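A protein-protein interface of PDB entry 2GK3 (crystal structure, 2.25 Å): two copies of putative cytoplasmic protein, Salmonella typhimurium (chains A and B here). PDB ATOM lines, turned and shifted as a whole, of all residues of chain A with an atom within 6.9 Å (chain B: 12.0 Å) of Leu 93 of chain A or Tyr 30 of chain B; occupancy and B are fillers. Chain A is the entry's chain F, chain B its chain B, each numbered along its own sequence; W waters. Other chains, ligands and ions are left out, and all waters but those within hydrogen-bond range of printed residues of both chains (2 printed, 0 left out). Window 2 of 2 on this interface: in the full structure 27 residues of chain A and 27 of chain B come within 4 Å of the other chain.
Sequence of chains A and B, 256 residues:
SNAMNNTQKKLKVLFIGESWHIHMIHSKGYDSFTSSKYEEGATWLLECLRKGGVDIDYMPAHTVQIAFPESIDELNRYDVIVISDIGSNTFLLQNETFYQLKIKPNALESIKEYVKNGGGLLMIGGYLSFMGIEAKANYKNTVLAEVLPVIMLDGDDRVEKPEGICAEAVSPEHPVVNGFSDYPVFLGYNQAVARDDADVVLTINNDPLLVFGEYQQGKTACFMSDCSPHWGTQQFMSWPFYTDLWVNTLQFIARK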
ATOM      1  N   ALA A  61      12.883  16.533  18.496  1.00  0.00           N
ATOM      2  CA  ALA A  61      11.846  15.759  19.210  1.00  0.00           C
ATOM      3  C   ALA A  61      10.578  15.550  18.383  1.00  0.00           C
ATOM      4  O   ALA A  61       9.994  14.463  18.393  1.00  0.00           O
ATOM      5  CB  ALA A  61      11.512  16.411  20.535  1.00  0.00           C
ATOM      6  N   HIS A  62      10.157  16.584  17.653  1.00  0.00           N
ATOM      7  CA  HIS A  62       8.970  16.450  16.810  1.00  0.00           C
ATOM      8  C   HIS A  62       9.155  15.432  15.699  1.00  0.00           C
ATOM      9  O   HIS A  62       8.178  14.806  15.280  1.00  0.00           O
ATOM     10  CB  HIS A  62       8.461  17.800  16.277  1.00  0.00           C
ATOM     11  CG  HIS A  62       9.476  18.592  15.504  1.00  0.00           C
ATOM     12  ND1 HIS A  62       9.885  18.247  14.231  1.00  0.00           N
ATOM     13  CD2 HIS A  62      10.131  19.735  15.810  1.00  0.00           C
ATOM     14  CE1 HIS A  62      10.769  19.129  13.799  1.00  0.00           C
ATOM     15  NE2 HIS A  62      10.932  20.045  14.737  1.00  0.00           N
ATOM     16  N   GLN A  65       8.256  11.948  16.926  1.00  0.00           N
ATOM     17  CA  GLN A  65       6.806  11.802  16.909  1.00  0.00           C
ATOM     18  C   GLN A  65       6.202  11.398  15.557  1.00  0.00           C
ATOM     19  O   GLN A  65       5.191  10.696  15.529  1.00  0.00           O
ATOM     20  CB  GLN A  65       6.163  13.109  17.330  1.00  0.00           C
ATOM     21  CG  GLN A  65       6.470  13.547  18.728  1.00  0.00           C
ATOM     22  CD  GLN A  65       5.579  14.686  19.131  1.00  0.00           C
ATOM     23  OE1 GLN A  65       5.658  15.757  18.550  1.00  0.00           O
ATOM     24  NE2 GLN A  65       4.691  14.452  20.090  1.00  0.00           N
ATOM     25  N   ILE A  86      14.786  14.900  25.834  1.00  0.00           N
ATOM     26  CA  ILE A  86      13.606  14.351  25.187  1.00  0.00           C
ATOM     27  C   ILE A  86      13.092  13.192  26.074  1.00  0.00           C
ATOM     28  O   ILE A  86      13.834  12.241  26.361  1.00  0.00           O
ATOM     29  CB  ILE A  86      13.910  13.941  23.717  1.00  0.00           C
ATOM     30  CG1 ILE A  86      12.656  13.379  23.045  1.00  0.00           C
ATOM     31  CG2 ILE A  86      15.174  13.022  23.636  1.00  0.00           C
ATOM     32  CD1 ILE A  86      12.871  12.862  21.707  1.00  0.00           C
ATOM     33  N   GLY A  87      11.847  13.305  26.545  1.00  0.00           N
ATOM     34  CA  GLY A  87      11.323  12.373  27.525  1.00  0.00           C
ATOM     35  C   GLY A  87      10.826  11.084  26.919  1.00  0.00           C
ATOM     36  O   GLY A  87      10.431  11.040  25.759  1.00  0.00           O
ATOM     37  N   SER A  88      10.837  10.035  27.717  1.00  0.00           N
ATOM     38  CA  SER A  88      10.305   8.737  27.306  1.00  0.00           C
ATOM     39  C   SER A  88       8.932   8.770  26.575  1.00  0.00           C
ATOM     40  O   SER A  88       8.721   7.972  25.677  1.00  0.00           O
ATOM     41  CB  SER A  88      10.264   7.767  28.497  1.00  0.00           C
ATOM     42  OG  SER A  88       9.356   8.197  29.496  1.00  0.00           O
ATOM     43  N   ASN A  89       8.033   9.682  26.956  1.00  0.00           N
ATOM     44  CA  ASN A  89       6.702   9.793  26.332  1.00  0.00           C
ATOM     45  C   ASN A  89       6.739  10.105  24.842  1.00  0.00           C
ATOM     46  O   ASN A  89       5.874   9.662  24.077  1.00  0.00           O
ATOM     47  CB  ASN A  89       5.828  10.843  27.051  1.00  0.00           C
ATOM     48  CG  ASN A  89       5.470  10.433  28.493  1.00  0.00           C
ATOM     49  OD1 ASN A  89       5.442   9.241  28.821  1.00  0.00           O
ATOM     50  ND2 ASN A  89       5.216  11.425  29.361  1.00  0.00           N
ATOM     51  N   THR A  90       7.736  10.892  24.436  1.00  0.00           N
ATOM     52  CA  THR A  90       7.924  11.225  23.027  1.00  0.00           C
ATOM     53  C   THR A  90       8.208   9.960  22.207  1.00  0.00           C
ATOM     54  O   THR A  90       7.643   9.810  21.153  1.00  0.00           O
ATOM     55  CB  THR A  90       9.003  12.318  22.845  1.00  0.00           C
ATOM     56  OG1 THR A  90       8.592  13.508  23.541  1.00  0.00           O
ATOM     57  CG2 THR A  90       9.183  12.668  21.391  1.00  0.00           C
ATOM     58  N   PHE A  91       9.041   9.045  22.701  1.00  0.00           N
ATOM     59  CA  PHE A  91       9.272   7.774  22.017  1.00  0.00           C
ATOM     60  C   PHE A  91       8.062   6.830  22.041  1.00  0.00           C
ATOM     61  O   PHE A  91       7.768   6.155  21.059  1.00  0.00           O
ATOM     62  CB  PHE A  91      10.489   7.051  22.609  1.00  0.00           C
ATOM     63  CG  PHE A  91      11.789   7.773  22.404  1.00  0.00           C
ATOM     64  CD1 PHE A  91      12.313   8.596  23.405  1.00  0.00           C
ATOM     65  CD2 PHE A  91      12.488   7.646  21.213  1.00  0.00           C
ATOM     66  CE1 PHE A  91      13.511   9.269  23.225  1.00  0.00           C
ATOM     67  CE2 PHE A  91      13.697   8.329  21.017  1.00  0.00           C
ATOM     68  CZ  PHE A  91      14.209   9.139  22.028  1.00  0.00           C
ATOM     69  N   LEU A  92       7.375   6.777  23.180  1.00  0.00           N
ATOM     70  CA  LEU A  92       6.339   5.767  23.409  1.00  0.00           C
ATOM     71  C   LEU A  92       5.004   6.187  22.854  1.00  0.00           C
ATOM     72  O   LEU A  92       4.217   5.322  22.428  1.00  0.00           O
ATOM     73  CB  LEU A  92       6.178   5.444  24.894  1.00  0.00           C
ATOM     74  CG  LEU A  92       7.360   4.746  25.563  1.00  0.00           C
ATOM     75  CD1 LEU A  92       7.350   5.011  27.081  1.00  0.00           C
ATOM     76  CD2 LEU A  92       7.375   3.265  25.238  1.00  0.00           C
ATOM     77  N   LEU A  93       4.753   7.497  22.863  1.00  0.00           N
ATOM     78  CA  LEU A  93       3.475   8.047  22.405  1.00  0.00           C
ATOM     79  C   LEU A  93       3.603   8.880  21.106  1.00  0.00           C
ATOM     80  O   LEU A  93       3.180  10.041  21.040  1.00  0.00           O
ATOM     81  CB  LEU A  93       2.794   8.820  23.541  1.00  0.00           C
ATOM     82  CG  LEU A  93       2.733   8.040  24.865  1.00  0.00           C
ATOM     83  CD1 LEU A  93       2.252   8.933  25.998  1.00  0.00           C
ATOM     84  CD2 LEU A  93       1.876   6.769  24.754  1.00  0.00           C
ATOM     85  N   GLN A  94       4.180   8.257  20.074  1.00  0.00           N
ATOM     86  CA  GLN A  94       4.253   8.859  18.727  1.00  0.00           C
ATOM     87  C   GLN A  94       2.846   9.174  18.219  1.00  0.00           C
ATOM     88  O   GLN A  94       1.867   8.619  18.728  1.00  0.00           O
ATOM     89  CB  GLN A  94       4.994   7.940  17.750  1.00  0.00           C
ATOM     90  CG  GLN A  94       6.485   7.761  18.074  1.00  0.00           C
ATOM     91  CD  GLN A  94       7.090   6.528  17.421  1.00  0.00           C
ATOM     92  OE1 GLN A  94       6.918   6.297  16.214  1.00  0.00           O
ATOM     93  NE2 GLN A  94       7.809   5.727  18.213  1.00  0.00           N
ATOM     94  N   ASN A  95       2.753  10.079  17.237  1.00  0.00           N
ATOM     95  CA  ASN A  95       1.463  10.622  16.788  1.00  0.00           C
ATOM     96  C   ASN A  95       0.505   9.561  16.271  1.00  0.00           C
ATOM     97  O   ASN A  95      -0.693   9.632  16.521  1.00  0.00           O
ATOM     98  CB  ASN A  95       1.646  11.735  15.755  1.00  0.00           C
ATOM     99  CG  ASN A  95       2.392  12.949  16.316  1.00  0.00           C
ATOM    100  OD1 ASN A  95       2.768  12.980  17.485  1.00  0.00           O
ATOM    101  ND2 ASN A  95       2.610  13.948  15.475  1.00  0.00           N
ATOM    102  N   GLU A  96       1.038   8.565  15.583  1.00  0.00           N
ATOM    103  CA  GLU A  96       0.205   7.472  15.095  1.00  0.00           C
ATOM    104  C   GLU A  96      -0.349   6.616  16.223  1.00  0.00           C
ATOM    105  O   GLU A  96      -1.426   6.029  16.094  1.00  0.00           O
ATOM    106  CB  GLU A  96       0.962   6.626  14.079  1.00  0.00           C
ATOM    107  CG  GLU A  96       0.937   7.247  12.699  1.00  0.00           C
ATOM    108  CD  GLU A  96       2.274   7.169  12.020  1.00  0.00           C
ATOM    109  OE1 GLU A  96       2.807   6.043  11.883  1.00  0.00           O
ATOM    110  OE2 GLU A  96       2.806   8.244  11.638  1.00  0.00           O
ATOM    111  N   THR A  97       0.395   6.558  17.323  1.00  0.00           N
ATOM    112  CA  THR A  97      -0.036   5.873  18.526  1.00  0.00           C
ATOM    113  C   THR A  97      -1.119   6.678  19.254  1.00  0.00           C
ATOM    114  O   THR A  97      -2.202   6.151  19.559  1.00  0.00           O
ATOM    115  CB  THR A  97       1.158   5.603  19.479  1.00  0.00           C
ATOM    116  OG1 THR A  97       2.023   4.612  18.911  1.00  0.00           O
ATOM    117  CG2 THR A  97       0.676   5.118  20.827  1.00  0.00           C
ATOM    118  N   PHE A  98      -0.831   7.946  19.520  1.00  0.00           N
ATOM    119  CA  PHE A  98      -1.664   8.721  20.419  1.00  0.00           C
ATOM    120  C   PHE A  98      -2.932   9.318  19.781  1.00  0.00           C
ATOM    121  O   PHE A  98      -3.944   9.541  20.465  1.00  0.00           O
ATOM    122  CB  PHE A  98      -0.851   9.798  21.138  1.00  0.00           C
ATOM    123  CG  PHE A  98      -1.520  10.311  22.382  1.00  0.00           C
ATOM    124  CD1 PHE A  98      -1.554   9.536  23.537  1.00  0.00           C
ATOM    125  CD2 PHE A  98      -2.138  11.552  22.395  1.00  0.00           C
ATOM    126  CE1 PHE A  98      -2.173   9.989  24.683  1.00  0.00           C
ATOM    127  CE2 PHE A  98      -2.776  12.020  23.543  1.00  0.00           C
ATOM    128  CZ  PHE A  98      -2.792  11.229  24.694  1.00  0.00           C
ATOM    129  N   TYR A  99      -2.871   9.594  18.487  1.00  0.00           N
ATOM    130  CA  TYR A  99      -3.964  10.281  17.816  1.00  0.00           C
ATOM    131  C   TYR A  99      -4.653   9.433  16.756  1.00  0.00           C
ATOM    132  O   TYR A  99      -5.853   9.519  16.611  1.00  0.00           O
ATOM    133  CB  TYR A  99      -3.473  11.593  17.190  1.00  0.00           C
ATOM    134  CG  TYR A  99      -2.888  12.550  18.191  1.00  0.00           C
ATOM    135  CD1 TYR A  99      -3.712  13.224  19.101  1.00  0.00           C
ATOM    136  CD2 TYR A  99      -1.511  12.768  18.246  1.00  0.00           C
ATOM    137  CE1 TYR A  99      -3.177  14.108  20.036  1.00  0.00           C
ATOM    138  CE2 TYR A  99      -0.959  13.663  19.180  1.00  0.00           C
ATOM    139  CZ  TYR A  99      -1.800  14.322  20.055  1.00  0.00           C
ATOM    140  OH  TYR A  99      -1.271  15.179  20.963  1.00  0.00           O
ATOM    141  N   ILE B  25       5.317  27.888  27.972  1.00  0.00           N
ATOM    142  CA  ILE B  25       5.074  26.466  27.803  1.00  0.00           C
ATOM    143  C   ILE B  25       6.172  25.931  26.887  1.00  0.00           C
ATOM    144  O   ILE B  25       6.221  26.244  25.688  1.00  0.00           O
ATOM    145  CB  ILE B  25       3.628  26.184  27.254  1.00  0.00           C
ATOM    146  CG1 ILE B  25       2.601  27.038  28.012  1.00  0.00           C
ATOM    147  CG2 ILE B  25       3.296  24.675  27.287  1.00  0.00           C
ATOM    148  CD1 ILE B  25       1.130  26.728  27.701  1.00  0.00           C
ATOM    149  N   HIS B  26       7.079  25.145  27.466  1.00  0.00           N
ATOM    150  CA  HIS B  26       8.192  24.597  26.719  1.00  0.00           C
ATOM    151  C   HIS B  26       7.817  23.181  26.324  1.00  0.00           C
ATOM    152  O   HIS B  26       7.932  22.275  27.143  1.00  0.00           O
ATOM    153  CB  HIS B  26       9.467  24.525  27.570  1.00  0.00           C
ATOM    154  CG  HIS B  26       9.808  25.771  28.335  1.00  0.00           C
ATOM    155  ND1 HIS B  26      10.911  26.550  28.034  1.00  0.00           N
ATOM    156  CD2 HIS B  26       9.269  26.310  29.456  1.00  0.00           C
ATOM    157  CE1 HIS B  26      11.011  27.534  28.907  1.00  0.00           C
ATOM    158  NE2 HIS B  26      10.023  27.414  29.779  1.00  0.00           N
ATOM    159  N   SER B  27       7.401  22.975  25.079  1.00  0.00           N
ATOM    160  CA  SER B  27       7.082  21.625  24.596  1.00  0.00           C
ATOM    161  C   SER B  27       8.279  20.955  23.929  1.00  0.00           C
ATOM    162  O   SER B  27       8.753  21.404  22.864  1.00  0.00           O
ATOM    163  CB  SER B  27       5.885  21.624  23.628  1.00  0.00           C
ATOM    164  OG  SER B  27       4.799  22.342  24.165  1.00  0.00           O
ATOM    165  N   LYS B  28       8.750  19.883  24.576  1.00  0.00           N
ATOM    166  CA  LYS B  28       9.777  19.002  24.062  1.00  0.00           C
ATOM    167  C   LYS B  28       9.066  17.727  23.635  1.00  0.00           C
ATOM    168  O   LYS B  28       8.840  16.850  24.450  1.00  0.00           O
ATOM    169  CB  LYS B  28      10.846  18.711  25.132  1.00  0.00           C
ATOM    170  CG  LYS B  28      11.403  19.951  25.899  1.00  0.00           C
ATOM    171  CD  LYS B  28      12.908  19.851  26.110  1.00  0.00           C
ATOM    172  CE  LYS B  28      13.446  20.616  27.333  1.00  0.00           C
ATOM    173  NZ  LYS B  28      13.405  22.092  27.194  1.00  0.00           N
ATOM    174  N   GLY B  29       8.695  17.631  22.357  1.00  0.00           N
ATOM    175  CA  GLY B  29       7.911  16.494  21.847  1.00  0.00           C
ATOM    176  C   GLY B  29       6.514  16.370  22.454  1.00  0.00           C
ATOM    177  O   GLY B  29       5.758  17.340  22.491  1.00  0.00           O
ATOM    178  N   TYR B  30       6.174  15.166  22.930  1.00  0.00           N
ATOM    179  CA  TYR B  30       4.888  14.906  23.591  1.00  0.00           C
ATOM    180  C   TYR B  30       4.696  15.782  24.816  1.00  0.00           C
ATOM    181  O   TYR B  30       3.610  16.318  25.040  1.00  0.00           O
ATOM    182  CB  TYR B  30       4.756  13.423  23.968  1.00  0.00           C
ATOM    183  CG  TYR B  30       3.442  13.080  24.643  1.00  0.00           C
ATOM    184  CD1 TYR B  30       2.362  12.578  23.912  1.00  0.00           C
ATOM    185  CD2 TYR B  30       3.268  13.277  26.013  1.00  0.00           C
ATOM    186  CE1 TYR B  30       1.129  12.275  24.547  1.00  0.00           C
ATOM    187  CE2 TYR B  30       2.060  12.987  26.643  1.00  0.00           C
ATOM    188  CZ  TYR B  30       1.003  12.484  25.903  1.00  0.00           C
ATOM    189  OH  TYR B  30      -0.167  12.181  26.546  1.00  0.00           O
ATOM    190  N   ASP B  31       5.772  15.936  25.587  1.00  0.00           N
ATOM    191  CA  ASP B  31       5.756  16.595  26.895  1.00  0.00           C
ATOM    192  C   ASP B  31       5.985  18.082  26.853  1.00  0.00           C
ATOM    193  O   ASP B  31       6.600  18.600  25.933  1.00  0.00           O
ATOM    194  CB  ASP B  31       6.855  16.005  27.780  1.00  0.00           C
ATOM    195  CG  ASP B  31       6.750  14.512  27.902  1.00  0.00           C
ATOM    196  OD1 ASP B  31       7.626  13.829  27.352  1.00  0.00           O
ATOM    197  OD2 ASP B  31       5.785  14.020  28.526  1.00  0.00           O
ATOM    198  N   SER B  32       5.517  18.755  27.892  1.00  0.00           N
ATOM    199  CA  SER B  32       5.834  20.140  28.087  1.00  0.00           C
ATOM    200  C   SER B  32       6.077  20.429  29.569  1.00  0.00           C
ATOM    201  O   SER B  32       5.455  19.828  30.452  1.00  0.00           O
ATOM    202  CB  SER B  32       4.728  21.042  27.492  1.00  0.00           C
ATOM    203  OG  SER B  32       3.808  21.463  28.499  1.00  0.00           O
ATOM    204  N   PHE B  33       7.008  21.335  29.837  1.00  0.00           N
ATOM    205  CA  PHE B  33       7.165  21.886  31.171  1.00  0.00           C
ATOM    206  C   PHE B  33       7.010  23.403  31.106  1.00  0.00           C
ATOM    207  O   PHE B  33       7.189  24.025  30.049  1.00  0.00           O
ATOM    208  CB  PHE B  33       8.497  21.462  31.811  1.00  0.00           C
ATOM    209  CG  PHE B  33       9.669  22.331  31.431  1.00  0.00           C
ATOM    210  CD1 PHE B  33       9.995  23.447  32.189  1.00  0.00           C
ATOM    211  CD2 PHE B  33      10.446  22.026  30.311  1.00  0.00           C
ATOM    212  CE1 PHE B  33      11.086  24.257  31.838  1.00  0.00           C
ATOM    213  CE2 PHE B  33      11.542  22.814  29.962  1.00  0.00           C
ATOM    214  CZ  PHE B  33      11.852  23.942  30.716  1.00  0.00           C
ATOM    215  N   THR B  34       6.669  23.996  32.236  1.00  0.00           N
ATOM    216  CA  THR B  34       6.347  25.399  32.276  1.00  0.00           C
ATOM    217  C   THR B  34       7.277  26.133  33.234  1.00  0.00           C
ATOM    218  O   THR B  34       7.792  25.563  34.194  1.00  0.00           O
ATOM    219  CB  THR B  34       4.843  25.636  32.636  1.00  0.00           C
ATOM    220  OG1 THR B  34       4.527  25.044  33.912  1.00  0.00           O
ATOM    221  CG2 THR B  34       3.945  25.006  31.598  1.00  0.00           C
HETATM  222  O   HOH W   1       9.419  14.782  25.690  1.00  0.00           O
HETATM  223  O   HOH W   2       8.196  11.743  28.964  1.00  0.00           O
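The side-chain hydroxyl (OG1) of Thr 90 of chain A is in hydrogen-bond range of the backbone carbonyl oxygen (O) of Lys 28 of chain B, at 3.5 Å. N of Tyr 30 of chain B sits close to NE2 of Gln 65 of chain A. N of Tyr 30 of chain B is in hydrogen-bond range of OG1 of Thr 90 of chain A (3.0 Å). The side-chain carboxylate (OD2) of Asp 31 of chain B sits at hydrogen-bond distance from the side-chain amide nitrogen (ND2) of Asn 89 of chain A (2.8 Å).
The backbone NH (N) of Asn 95 of chain A lies within hydrogen-bond range of the backbone carbonyl oxygen (O) of Gln 65 of chain A (3.0 Å).
Among the printed residues, pairs that only touch across the chains: Phe 98 of chain A with Tyr 30 of chain B (3.4 Å), Thr 90 of chain A with Gly 29 of chain B (3.5 Å), Gln 65 of chain A with Gly 29 of chain B (3.5 Å), Ala 61 of chain A with Gly 29 of chain B (3.6 Å), Asn 89 of chain A with Tyr 30 of chain B (3.7 Å), Leu 93 of chain A with Tyr 30 of chain B (3.8 Å), Thr 90 of chain A with Asp 31 of chain B (3.9 Å) and Gly 87 of chain A with Asp 31 of chain B (3.98 Å).
Leu 93 of chain A touches just one residue of chain B: Tyr 30. Tyr 30 of chain B touches just these residues of chain A: Gln 65 (3.3 Å), Asn 89 (3.7 Å), Thr 90 (3.0 Å), Leu 93 (3.8 Å) and Phe 98 (3.4 Å). Gln 65 of chain A touches two residues of chain B. Gly 87 of chain A touches one residue of chain B. Asn 89 of chain A touches just these residues of chain B: Tyr 30 and Asp 31. No residue of chain B comes within 4 Å of Gln 94 of chain A. No residue of chain B comes within 4 Å of Asn 95 of chain A. No residue of chain B comes within 4 Å of Thr 97 of chain A. Phe 98 of chain A touches just one residue of chain B: Tyr 30. Printed residues of chain A within 4 Å of Gly 29 of chain B: Ala 61, Gln 65 and Thr 90. Printed residues of chain A within 4 Å of Asp 31 of chain B: Gly 87, Asn 89 and Thr 90. Thr 34 of chain B touches none of the printed residues of chain A. Glu 96 of chain A touches none of the printed residues of chain B. The nearest residue of chain A that does not touch Tyr 30 of chain B is Tyr 99 of chain A (5.2 Å). The nearest printed residue of chain A that does not touch Asp 31 of chain B is Ser 88 of chain A (5.0 Å).
Of the 10 printed residues of chain B, 4 touch a printed residue of chain A. Hydrophobic or aromatic side chains of chain B within 4 Å of the printed part of chain A: Tyr 30. Among the printed residues, 12 pairs touch across the chains. Among the printed residues, no Asp or Glu carboxylate lies within 4 Å of a Lys or Arg side-chain nitrogen of the other chain.
No position is printed for both chains.
Water W1 lies within hydrogen-bond range of O of Lys 28 of chain B (2.5 Å), OD1 of Asp 31 of chain B (2.6 Å), OG1 of Thr 90 of chain A (2.6 Å) and N of Gly 87 of chain A (3.0 Å). Water W2 lies within hydrogen-bond range of OD1 of Asp 31 of chain B (2.7 Å), N of Asn 89 of chain A (2.9 Å) and N of Ser 88 of chain A (3.4 Å).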
